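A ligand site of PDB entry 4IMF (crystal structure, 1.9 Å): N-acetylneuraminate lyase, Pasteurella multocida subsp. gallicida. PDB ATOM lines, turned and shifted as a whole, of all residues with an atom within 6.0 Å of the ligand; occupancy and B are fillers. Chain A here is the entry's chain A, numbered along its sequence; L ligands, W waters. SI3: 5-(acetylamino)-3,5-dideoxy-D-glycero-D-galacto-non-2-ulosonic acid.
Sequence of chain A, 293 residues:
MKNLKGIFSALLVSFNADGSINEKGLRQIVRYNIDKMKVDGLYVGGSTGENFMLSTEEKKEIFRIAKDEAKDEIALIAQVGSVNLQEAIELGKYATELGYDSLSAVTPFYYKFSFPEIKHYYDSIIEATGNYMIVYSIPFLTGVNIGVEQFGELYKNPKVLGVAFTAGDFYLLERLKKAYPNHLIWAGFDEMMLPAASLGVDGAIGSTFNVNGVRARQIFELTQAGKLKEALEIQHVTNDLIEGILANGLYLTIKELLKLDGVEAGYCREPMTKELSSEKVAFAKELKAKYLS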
ATOM      1  N   ALA A  10      14.181 -17.204  -3.023  1.00  0.00           N
ATOM      2  CA  ALA A  10      14.250 -17.575  -4.433  1.00  0.00           C
ATOM      3  C   ALA A  10      15.074 -18.856  -4.397  1.00  0.00           C
ATOM      4  O   ALA A  10      16.284 -18.830  -4.126  1.00  0.00           O
ATOM      5  CB  ALA A  10      14.912 -16.502  -5.257  1.00  0.00           C
ATOM      6  N   TYR A  43      10.007 -19.043  -4.057  1.00  0.00           N
ATOM      7  CA  TYR A  43       9.810 -18.578  -5.417  1.00  0.00           C
ATOM      8  C   TYR A  43      10.700 -19.503  -6.219  1.00  0.00           C
ATOM      9  O   TYR A  43      11.941 -19.403  -6.140  1.00  0.00           O
ATOM     10  CB  TYR A  43      10.259 -17.126  -5.480  1.00  0.00           C
ATOM     11  CG  TYR A  43      10.036 -16.397  -6.757  1.00  0.00           C
ATOM     12  CD1 TYR A  43      11.055 -16.290  -7.701  1.00  0.00           C
ATOM     13  CD2 TYR A  43       8.786 -15.753  -7.008  1.00  0.00           C
ATOM     14  CE1 TYR A  43      10.852 -15.564  -8.884  1.00  0.00           C
ATOM     15  CE2 TYR A  43       8.588 -15.062  -8.189  1.00  0.00           C
ATOM     16  CZ  TYR A  43       9.608 -14.950  -9.100  1.00  0.00           C
ATOM     17  OH  TYR A  43       9.414 -14.273 -10.279  1.00  0.00           O
ATOM     18  N   GLY A  45      12.018 -21.394  -9.755  1.00  0.00           N
ATOM     19  CA  GLY A  45      12.240 -21.128 -11.196  1.00  0.00           C
ATOM     20  C   GLY A  45      12.655 -19.721 -11.563  1.00  0.00           C
ATOM     21  O   GLY A  45      12.638 -19.334 -12.755  1.00  0.00           O
ATOM     22  N   GLY A  46      13.072 -18.958 -10.557  1.00  0.00           N
ATOM     23  CA  GLY A  46      13.522 -17.580 -10.780  1.00  0.00           C
ATOM     24  C   GLY A  46      14.947 -17.558 -11.326  1.00  0.00           C
ATOM     25  O   GLY A  46      15.511 -18.626 -11.589  1.00  0.00           O
ATOM     26  N   SER A  47      15.485 -16.354 -11.546  1.00  0.00           N
ATOM     27  CA  SER A  47      16.904 -16.174 -12.021  1.00  0.00           C
ATOM     28  C   SER A  47      17.869 -16.951 -11.075  1.00  0.00           C
ATOM     29  O   SER A  47      18.790 -17.608 -11.576  1.00  0.00           O
ATOM     30  CB  SER A  47      17.292 -14.709 -12.065  1.00  0.00           C
ATOM     31  OG  SER A  47      16.332 -13.962 -12.847  1.00  0.00           O
ATOM     32  N   THR A  48      17.630 -16.833  -9.751  1.00  0.00           N
ATOM     33  CA  THR A  48      18.443 -17.494  -8.694  1.00  0.00           C
ATOM     34  C   THR A  48      18.448 -19.029  -8.828  1.00  0.00           C
ATOM     35  O   THR A  48      19.421 -19.675  -8.482  1.00  0.00           O
ATOM     36  CB  THR A  48      17.905 -17.100  -7.276  1.00  0.00           C
ATOM     37  OG1 THR A  48      18.057 -15.683  -7.123  1.00  0.00           O
ATOM     38  CG2 THR A  48      18.725 -17.750  -6.163  1.00  0.00           C
ATOM     39  N   GLY A  49      17.366 -19.617  -9.345  1.00  0.00           N
ATOM     40  CA  GLY A  49      17.373 -21.056  -9.597  1.00  0.00           C
ATOM     41  C   GLY A  49      18.077 -21.482 -10.874  1.00  0.00           C
ATOM     42  O   GLY A  49      17.970 -22.669 -11.259  1.00  0.00           O
ATOM     43  N   TYR A 136       7.112 -10.362 -13.006  1.00  0.00           N
ATOM     44  CA  TYR A 136       8.523 -10.430 -12.461  1.00  0.00           C
ATOM     45  C   TYR A 136       9.312  -9.387 -13.256  1.00  0.00           C
ATOM     46  O   TYR A 136       9.581  -9.561 -14.460  1.00  0.00           O
ATOM     47  CB  TYR A 136       9.048 -11.850 -12.638  1.00  0.00           C
ATOM     48  CG  TYR A 136      10.510 -12.125 -12.254  1.00  0.00           C
ATOM     49  CD1 TYR A 136      11.160 -13.196 -12.858  1.00  0.00           C
ATOM     50  CD2 TYR A 136      11.210 -11.360 -11.298  1.00  0.00           C
ATOM     51  CE1 TYR A 136      12.490 -13.549 -12.514  1.00  0.00           C
ATOM     52  CE2 TYR A 136      12.532 -11.708 -10.957  1.00  0.00           C
ATOM     53  CZ  TYR A 136      13.165 -12.789 -11.590  1.00  0.00           C
ATOM     54  OH  TYR A 136      14.498 -13.182 -11.277  1.00  0.00           O
ATOM     55  N   ILE A 138      12.660  -7.268 -13.625  1.00  0.00           N
ATOM     56  CA  ILE A 138      14.113  -7.289 -13.333  1.00  0.00           C
ATOM     57  C   ILE A 138      14.883  -6.546 -14.413  1.00  0.00           C
ATOM     58  O   ILE A 138      15.639  -7.163 -15.227  1.00  0.00           O
ATOM     59  CB  ILE A 138      14.572  -8.757 -12.988  1.00  0.00           C
ATOM     60  CG1 ILE A 138      16.048  -8.817 -12.536  1.00  0.00           C
ATOM     61  CG2 ILE A 138      14.255  -9.749 -14.092  1.00  0.00           C
ATOM     62  CD1 ILE A 138      16.381 -10.225 -12.004  1.00  0.00           C
ATOM     63  N   PHE A 140      17.597  -4.809 -14.501  1.00  0.00           N
ATOM     64  CA  PHE A 140      19.068  -4.845 -14.696  1.00  0.00           C
ATOM     65  C   PHE A 140      19.525  -6.081 -15.514  1.00  0.00           C
ATOM     66  O   PHE A 140      20.673  -6.111 -16.062  1.00  0.00           O
ATOM     67  CB  PHE A 140      19.811  -4.679 -13.341  1.00  0.00           C
ATOM     68  CG  PHE A 140      20.046  -5.965 -12.613  1.00  0.00           C
ATOM     69  CD1 PHE A 140      18.993  -6.640 -11.968  1.00  0.00           C
ATOM     70  CD2 PHE A 140      21.343  -6.518 -12.570  1.00  0.00           C
ATOM     71  CE1 PHE A 140      19.235  -7.828 -11.249  1.00  0.00           C
ATOM     72  CE2 PHE A 140      21.584  -7.692 -11.862  1.00  0.00           C
ATOM     73  CZ  PHE A 140      20.564  -8.349 -11.215  1.00  0.00           C
ATOM     74  N   LEU A 141      18.666  -7.109 -15.606  1.00  0.00           N
ATOM     75  CA  LEU A 141      18.891  -8.250 -16.495  1.00  0.00           C
ATOM     76  C   LEU A 141      18.133  -8.175 -17.858  1.00  0.00           C
ATOM     77  O   LEU A 141      18.698  -8.581 -18.878  1.00  0.00           O
ATOM     78  CB  LEU A 141      18.578  -9.595 -15.853  1.00  0.00           C
ATOM     79  CG  LEU A 141      19.431  -9.886 -14.590  1.00  0.00           C
ATOM     80  CD1 LEU A 141      19.206 -11.340 -14.192  1.00  0.00           C
ATOM     81  CD2 LEU A 141      20.940  -9.626 -14.794  1.00  0.00           C
ATOM     82  N   THR A 166      12.376  -6.635  -8.596  1.00  0.00           N
ATOM     83  CA  THR A 166      13.856  -6.689  -8.508  1.00  0.00           C
ATOM     84  C   THR A 166      14.413  -5.500  -9.278  1.00  0.00           C
ATOM     85  O   THR A 166      14.990  -5.617 -10.339  1.00  0.00           O
ATOM     86  CB  THR A 166      14.382  -8.056  -9.007  1.00  0.00           C
ATOM     87  OG1 THR A 166      13.672  -9.126  -8.331  1.00  0.00           O
ATOM     88  CG2 THR A 166      15.890  -8.175  -8.746  1.00  0.00           C
ATOM     89  N   ALA A 187       9.768  -6.852  -2.667  1.00  0.00           N
ATOM     90  CA  ALA A 187      11.079  -6.278  -2.952  1.00  0.00           C
ATOM     91  C   ALA A 187      12.003  -7.413  -3.394  1.00  0.00           C
ATOM     92  O   ALA A 187      11.943  -8.484  -2.816  1.00  0.00           O
ATOM     93  CB  ALA A 187      11.646  -5.591  -1.704  1.00  0.00           C
ATOM     94  N   GLY A 188      12.863  -7.128  -4.370  1.00  0.00           N
ATOM     95  CA  GLY A 188      13.746  -8.130  -4.958  1.00  0.00           C
ATOM     96  C   GLY A 188      15.210  -7.914  -4.653  1.00  0.00           C
ATOM     97  O   GLY A 188      16.027  -8.859  -4.881  1.00  0.00           O
ATOM     98  N   PHE A 189      15.585  -6.728  -4.130  1.00  0.00           N
ATOM     99  CA  PHE A 189      17.038  -6.569  -3.786  1.00  0.00           C
ATOM    100  C   PHE A 189      17.227  -6.625  -2.260  1.00  0.00           C
ATOM    101  O   PHE A 189      16.841  -5.706  -1.529  1.00  0.00           O
ATOM    102  CB  PHE A 189      17.629  -5.275  -4.350  1.00  0.00           C
ATOM    103  CG  PHE A 189      17.937  -5.332  -5.830  1.00  0.00           C
ATOM    104  CD1 PHE A 189      17.327  -4.439  -6.702  1.00  0.00           C
ATOM    105  CD2 PHE A 189      18.791  -6.320  -6.355  1.00  0.00           C
ATOM    106  CE1 PHE A 189      17.575  -4.499  -8.065  1.00  0.00           C
ATOM    107  CE2 PHE A 189      19.035  -6.367  -7.720  1.00  0.00           C
ATOM    108  CZ  PHE A 189      18.466  -5.420  -8.565  1.00  0.00           C
ATOM    109  N   ASP A 190      17.800  -7.742  -1.798  1.00  0.00           N
ATOM    110  CA  ASP A 190      17.929  -8.054  -0.369  1.00  0.00           C
ATOM    111  C   ASP A 190      18.735  -6.974   0.346  1.00  0.00           C
ATOM    112  O   ASP A 190      18.480  -6.702   1.522  1.00  0.00           O
ATOM    113  CB  ASP A 190      18.690  -9.387  -0.185  1.00  0.00           C
ATOM    114  CG  ASP A 190      18.150 -10.556  -1.021  1.00  0.00           C
ATOM    115  OD1 ASP A 190      17.295 -10.395  -1.907  1.00  0.00           O
ATOM    116  OD2 ASP A 190      18.673 -11.703  -0.836  1.00  0.00           O
ATOM    117  N   GLU A 191      19.699  -6.381  -0.366  1.00  0.00           N
ATOM    118  CA  GLU A 191      20.622  -5.378   0.224  1.00  0.00           C
ATOM    119  C   GLU A 191      19.929  -4.005   0.282  1.00  0.00           C
ATOM    120  O   GLU A 191      20.513  -3.046   0.793  1.00  0.00           O
ATOM    121  CB  GLU A 191      21.933  -5.270  -0.583  1.00  0.00           C
ATOM    122  CG  GLU A 191      21.756  -4.924  -2.085  1.00  0.00           C
ATOM    123  CD  GLU A 191      21.561  -6.198  -2.966  1.00  0.00           C
ATOM    124  OE1 GLU A 191      20.824  -7.147  -2.602  1.00  0.00           O
ATOM    125  OE2 GLU A 191      22.178  -6.252  -4.045  1.00  0.00           O
ATOM    126  N   ILE A 205      11.338 -11.234  -2.082  1.00  0.00           N
ATOM    127  CA  ILE A 205      11.858 -12.468  -2.693  1.00  0.00           C
ATOM    128  C   ILE A 205      13.383 -12.315  -2.836  1.00  0.00           C
ATOM    129  O   ILE A 205      13.850 -11.344  -3.457  1.00  0.00           O
ATOM    130  CB  ILE A 205      11.220 -12.687  -4.081  1.00  0.00           C
ATOM    131  CG1 ILE A 205       9.717 -12.987  -3.917  1.00  0.00           C
ATOM    132  CG2 ILE A 205      11.923 -13.819  -4.868  1.00  0.00           C
ATOM    133  CD1 ILE A 205       8.863 -12.566  -5.096  1.00  0.00           C
ATOM    134  N   GLY A 206      14.167 -13.245  -2.272  1.00  0.00           N
ATOM    135  CA  GLY A 206      15.599 -13.059  -2.226  1.00  0.00           C
ATOM    136  C   GLY A 206      16.406 -14.373  -2.283  1.00  0.00           C
ATOM    137  O   GLY A 206      16.031 -15.411  -1.711  1.00  0.00           O
ATOM    138  N   SER A 207      17.521 -14.271  -2.995  1.00  0.00           N
ATOM    139  CA  SER A 207      18.500 -15.387  -3.040  1.00  0.00           C
ATOM    140  C   SER A 207      19.152 -15.579  -1.685  1.00  0.00           C
ATOM    141  O   SER A 207      19.442 -16.730  -1.249  1.00  0.00           O
ATOM    142  CB  SER A 207      19.607 -15.038  -4.069  1.00  0.00           C
ATOM    143  OG  SER A 207      20.377 -13.900  -3.670  1.00  0.00           O
ATOM    144  N   THR A 208      19.469 -14.468  -1.023  1.00  0.00           N
ATOM    145  CA  THR A 208      20.297 -14.617   0.185  1.00  0.00           C
ATOM    146  C   THR A 208      19.480 -15.154   1.352  1.00  0.00           C
ATOM    147  O   THR A 208      20.070 -15.597   2.384  1.00  0.00           O
ATOM    148  CB  THR A 208      21.083 -13.318   0.579  1.00  0.00           C
ATOM    149  OG1 THR A 208      20.207 -12.303   1.073  1.00  0.00           O
ATOM    150  CG2 THR A 208      21.984 -12.846  -0.554  1.00  0.00           C
ATOM    151  N   ILE A 242      26.347  -9.745   2.293  1.00  0.00           N
ATOM    152  CA  ILE A 242      25.970  -9.676   0.865  1.00  0.00           C
ATOM    153  C   ILE A 242      27.109  -9.096   0.029  1.00  0.00           C
ATOM    154  O   ILE A 242      27.413  -9.648  -1.007  1.00  0.00           O
ATOM    155  CB  ILE A 242      24.613  -8.925   0.603  1.00  0.00           C
ATOM    156  CG1 ILE A 242      23.444  -9.654   1.289  1.00  0.00           C
ATOM    157  CG2 ILE A 242      24.390  -8.722  -0.916  1.00  0.00           C
ATOM    158  CD1 ILE A 242      22.097  -8.873   1.279  1.00  0.00           C
ATOM    159  N   LEU A 246      28.553 -11.280  -3.036  1.00  0.00           N
ATOM    160  CA  LEU A 246      28.651 -10.728  -4.389  1.00  0.00           C
ATOM    161  C   LEU A 246      30.108 -10.719  -4.880  1.00  0.00           C
ATOM    162  O   LEU A 246      30.367 -11.018  -6.043  1.00  0.00           O
ATOM    163  CB  LEU A 246      28.067  -9.257  -4.418  1.00  0.00           C
ATOM    164  CG  LEU A 246      26.535  -9.268  -4.311  1.00  0.00           C
ATOM    165  CD1 LEU A 246      25.967  -7.847  -4.086  1.00  0.00           C
ATOM    166  CD2 LEU A 246      25.876  -9.875  -5.586  1.00  0.00           C
ATOM    167  N   LEU A 250      28.096 -14.855  -6.427  1.00  0.00           N
ATOM    168  CA  LEU A 250      26.806 -14.978  -5.783  1.00  0.00           C
ATOM    169  C   LEU A 250      26.168 -16.367  -5.580  1.00  0.00           C
ATOM    170  O   LEU A 250      25.991 -16.805  -4.421  1.00  0.00           O
ATOM    171  CB  LEU A 250      25.817 -14.002  -6.525  1.00  0.00           C
ATOM    172  CG  LEU A 250      24.337 -13.981  -6.087  1.00  0.00           C
ATOM    173  CD1 LEU A 250      24.130 -13.495  -4.658  1.00  0.00           C
ATOM    174  CD2 LEU A 250      23.580 -12.974  -7.040  1.00  0.00           C
ATOM    175  N   TYR A 251      25.743 -17.036  -6.654  1.00  0.00           N
ATOM    176  CA  TYR A 251      25.064 -18.310  -6.501  1.00  0.00           C
ATOM    177  C   TYR A 251      25.998 -19.369  -5.908  1.00  0.00           C
ATOM    178  O   TYR A 251      25.560 -20.126  -5.052  1.00  0.00           O
ATOM    179  CB  TYR A 251      24.440 -18.796  -7.795  1.00  0.00           C
ATOM    180  CG  TYR A 251      23.440 -17.719  -8.317  1.00  0.00           C
ATOM    181  CD1 TYR A 251      22.609 -16.981  -7.426  1.00  0.00           C
ATOM    182  CD2 TYR A 251      23.352 -17.451  -9.665  1.00  0.00           C
ATOM    183  CE1 TYR A 251      21.714 -15.983  -7.895  1.00  0.00           C
ATOM    184  CE2 TYR A 251      22.461 -16.443 -10.133  1.00  0.00           C
ATOM    185  CZ  TYR A 251      21.646 -15.754  -9.256  1.00  0.00           C
ATOM    186  OH  TYR A 251      20.779 -14.756  -9.736  1.00  0.00           O
ATOM    187  N   ILE A 254      26.392 -18.641  -2.010  1.00  0.00           N
ATOM    188  CA  ILE A 254      25.233 -19.056  -1.237  1.00  0.00           C
ATOM    189  C   ILE A 254      25.204 -20.585  -1.126  1.00  0.00           C
ATOM    190  O   ILE A 254      24.963 -21.136  -0.044  1.00  0.00           O
ATOM    191  CB  ILE A 254      23.884 -18.546  -1.805  1.00  0.00           C
ATOM    192  CG1 ILE A 254      23.897 -17.004  -1.889  1.00  0.00           C
ATOM    193  CG2 ILE A 254      22.771 -18.886  -0.810  1.00  0.00           C
ATOM    194  CD1 ILE A 254      22.767 -16.410  -2.748  1.00  0.00           C
HETATM  195  O1A SI3 L   1      14.962 -15.481  -8.729  1.00  0.00           O
HETATM  196  C1  SI3 L   1      15.740 -14.485  -8.626  1.00  0.00           C
HETATM  197  O1B SI3 L   1      16.808 -14.614  -9.161  1.00  0.00           O
HETATM  198  C2  SI3 L   1      15.444 -13.202  -8.121  1.00  0.00           C
HETATM  199  O2  SI3 L   1      15.262 -12.334  -9.018  1.00  0.00           O
HETATM  200  C3  SI3 L   1      15.372 -13.023  -6.625  1.00  0.00           C
HETATM  201  C4  SI3 L   1      16.128 -11.825  -6.081  1.00  0.00           C
HETATM  202  O4  SI3 L   1      15.552 -10.707  -6.802  1.00  0.00           O
HETATM  203  C5  SI3 L   1      17.647 -11.884  -6.397  1.00  0.00           C
HETATM  204  N5  SI3 L   1      17.918 -11.480  -7.809  1.00  0.00           N
HETATM  205  C10 SI3 L   1      18.848 -12.086  -8.566  1.00  0.00           C
HETATM  206  C11 SI3 L   1      18.884 -11.773 -10.048  1.00  0.00           C
HETATM  207  O10 SI3 L   1      19.667 -12.905  -8.031  1.00  0.00           O
HETATM  208  C6  SI3 L   1      18.315 -10.977  -5.412  1.00  0.00           C
HETATM  209  O6  SI3 L   1      17.942 -11.613  -4.198  1.00  0.00           O
HETATM  210  C7  SI3 L   1      19.852 -10.809  -5.475  1.00  0.00           C
HETATM  211  O7  SI3 L   1      20.375 -12.114  -5.676  1.00  0.00           O
HETATM  212  C8  SI3 L   1      20.475 -10.154  -4.258  1.00  0.00           C
HETATM  213  O8  SI3 L   1      19.656  -9.006  -3.850  1.00  0.00           O
HETATM  214  C9  SI3 L   1      21.889  -9.645  -4.437  1.00  0.00           C
HETATM  215  O9  SI3 L   1      21.969  -8.858  -5.617  1.00  0.00           O
HETATM  216  O   HOH W   1      22.246  -9.076  -8.161  1.00  0.00           O
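OD2 of Asp 190 sits at hydrogen-bond distance from OG1 of Thr 208 (2.5 Å).
The side-chain hydroxyl of Tyr 136 is in hydrogen-bond range of the side-chain hydroxyl of Ser 47 (2.5 Å).
O of Ala 187 lies within hydrogen-bond range of N of Ile 205 (2.9 Å).
The backbone carbonyl oxygen of Gly 206 lies within hydrogen-bond range of the backbone NH of Ala 10, at 2.9 Å.
The backbone carbonyl oxygen (O) of Gly 188 is in hydrogen-bond range of an oxygen (O4) of the ligand (2.7 Å).
The side-chain hydroxyl of Ser 207 sits at hydrogen-bond distance from an oxygen (O7) of the ligand (2.7 Å).
The side-chain hydroxyl of Tyr 251 lies within hydrogen-bond range of an oxygen (O10) of the ligand (2.8 Å).
The backbone NH (N) of Thr 48 is in hydrogen-bond range of an oxygen (O1B) of the ligand, at 2.4 Å.
An oxygen (O8) of the ligand lies within hydrogen-bond range of the backbone NH (N) of Asp 190, 3.0 Å away.
An oxygen (O6) of the ligand sits at hydrogen-bond distance from the side-chain carboxylate (OD1) of Asp 190.
OE1 of Glu 191 is in hydrogen-bond range of O8 of the ligand (2.5 Å).
An oxygen (O1B) of the ligand is in hydrogen-bond range of the side-chain hydroxyl (OG1) of Thr 48, 2.6 Å away.
N of Ser 207 lies within hydrogen-bond range of O6 of the ligand (2.9 Å).
An oxygen (O4) of the ligand sits at hydrogen-bond distance from the side-chain hydroxyl (OG1) of Thr 166 (2.9 Å).
An oxygen (O1A) of the ligand is in hydrogen-bond range of the backbone NH (N) of Ser 47 (3.0 Å).
OH of Tyr 136 sits at hydrogen-bond distance from O2 of the ligand (2.5 Å).
Residues that only touch the ligand: Ala 10 (3.6 Å), Gly 46 (3.3 Å), Ile 138 (3.5 Å), Phe 140 (3.99 Å), Phe 189 (3.6 Å), Ile 205 (3.5 Å), Gly 206 (3.4 Å) and Leu 250 (3.6 Å).
Hydrophobic or aromatic side chains within 4 Å of the ligand: Ala 10, Tyr 136, Ile 138, Phe 140, Phe 189, Ile 205, Leu 250 and Tyr 251.
Of the 26 residues printed, 17 come within 4 Å of the ligand.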
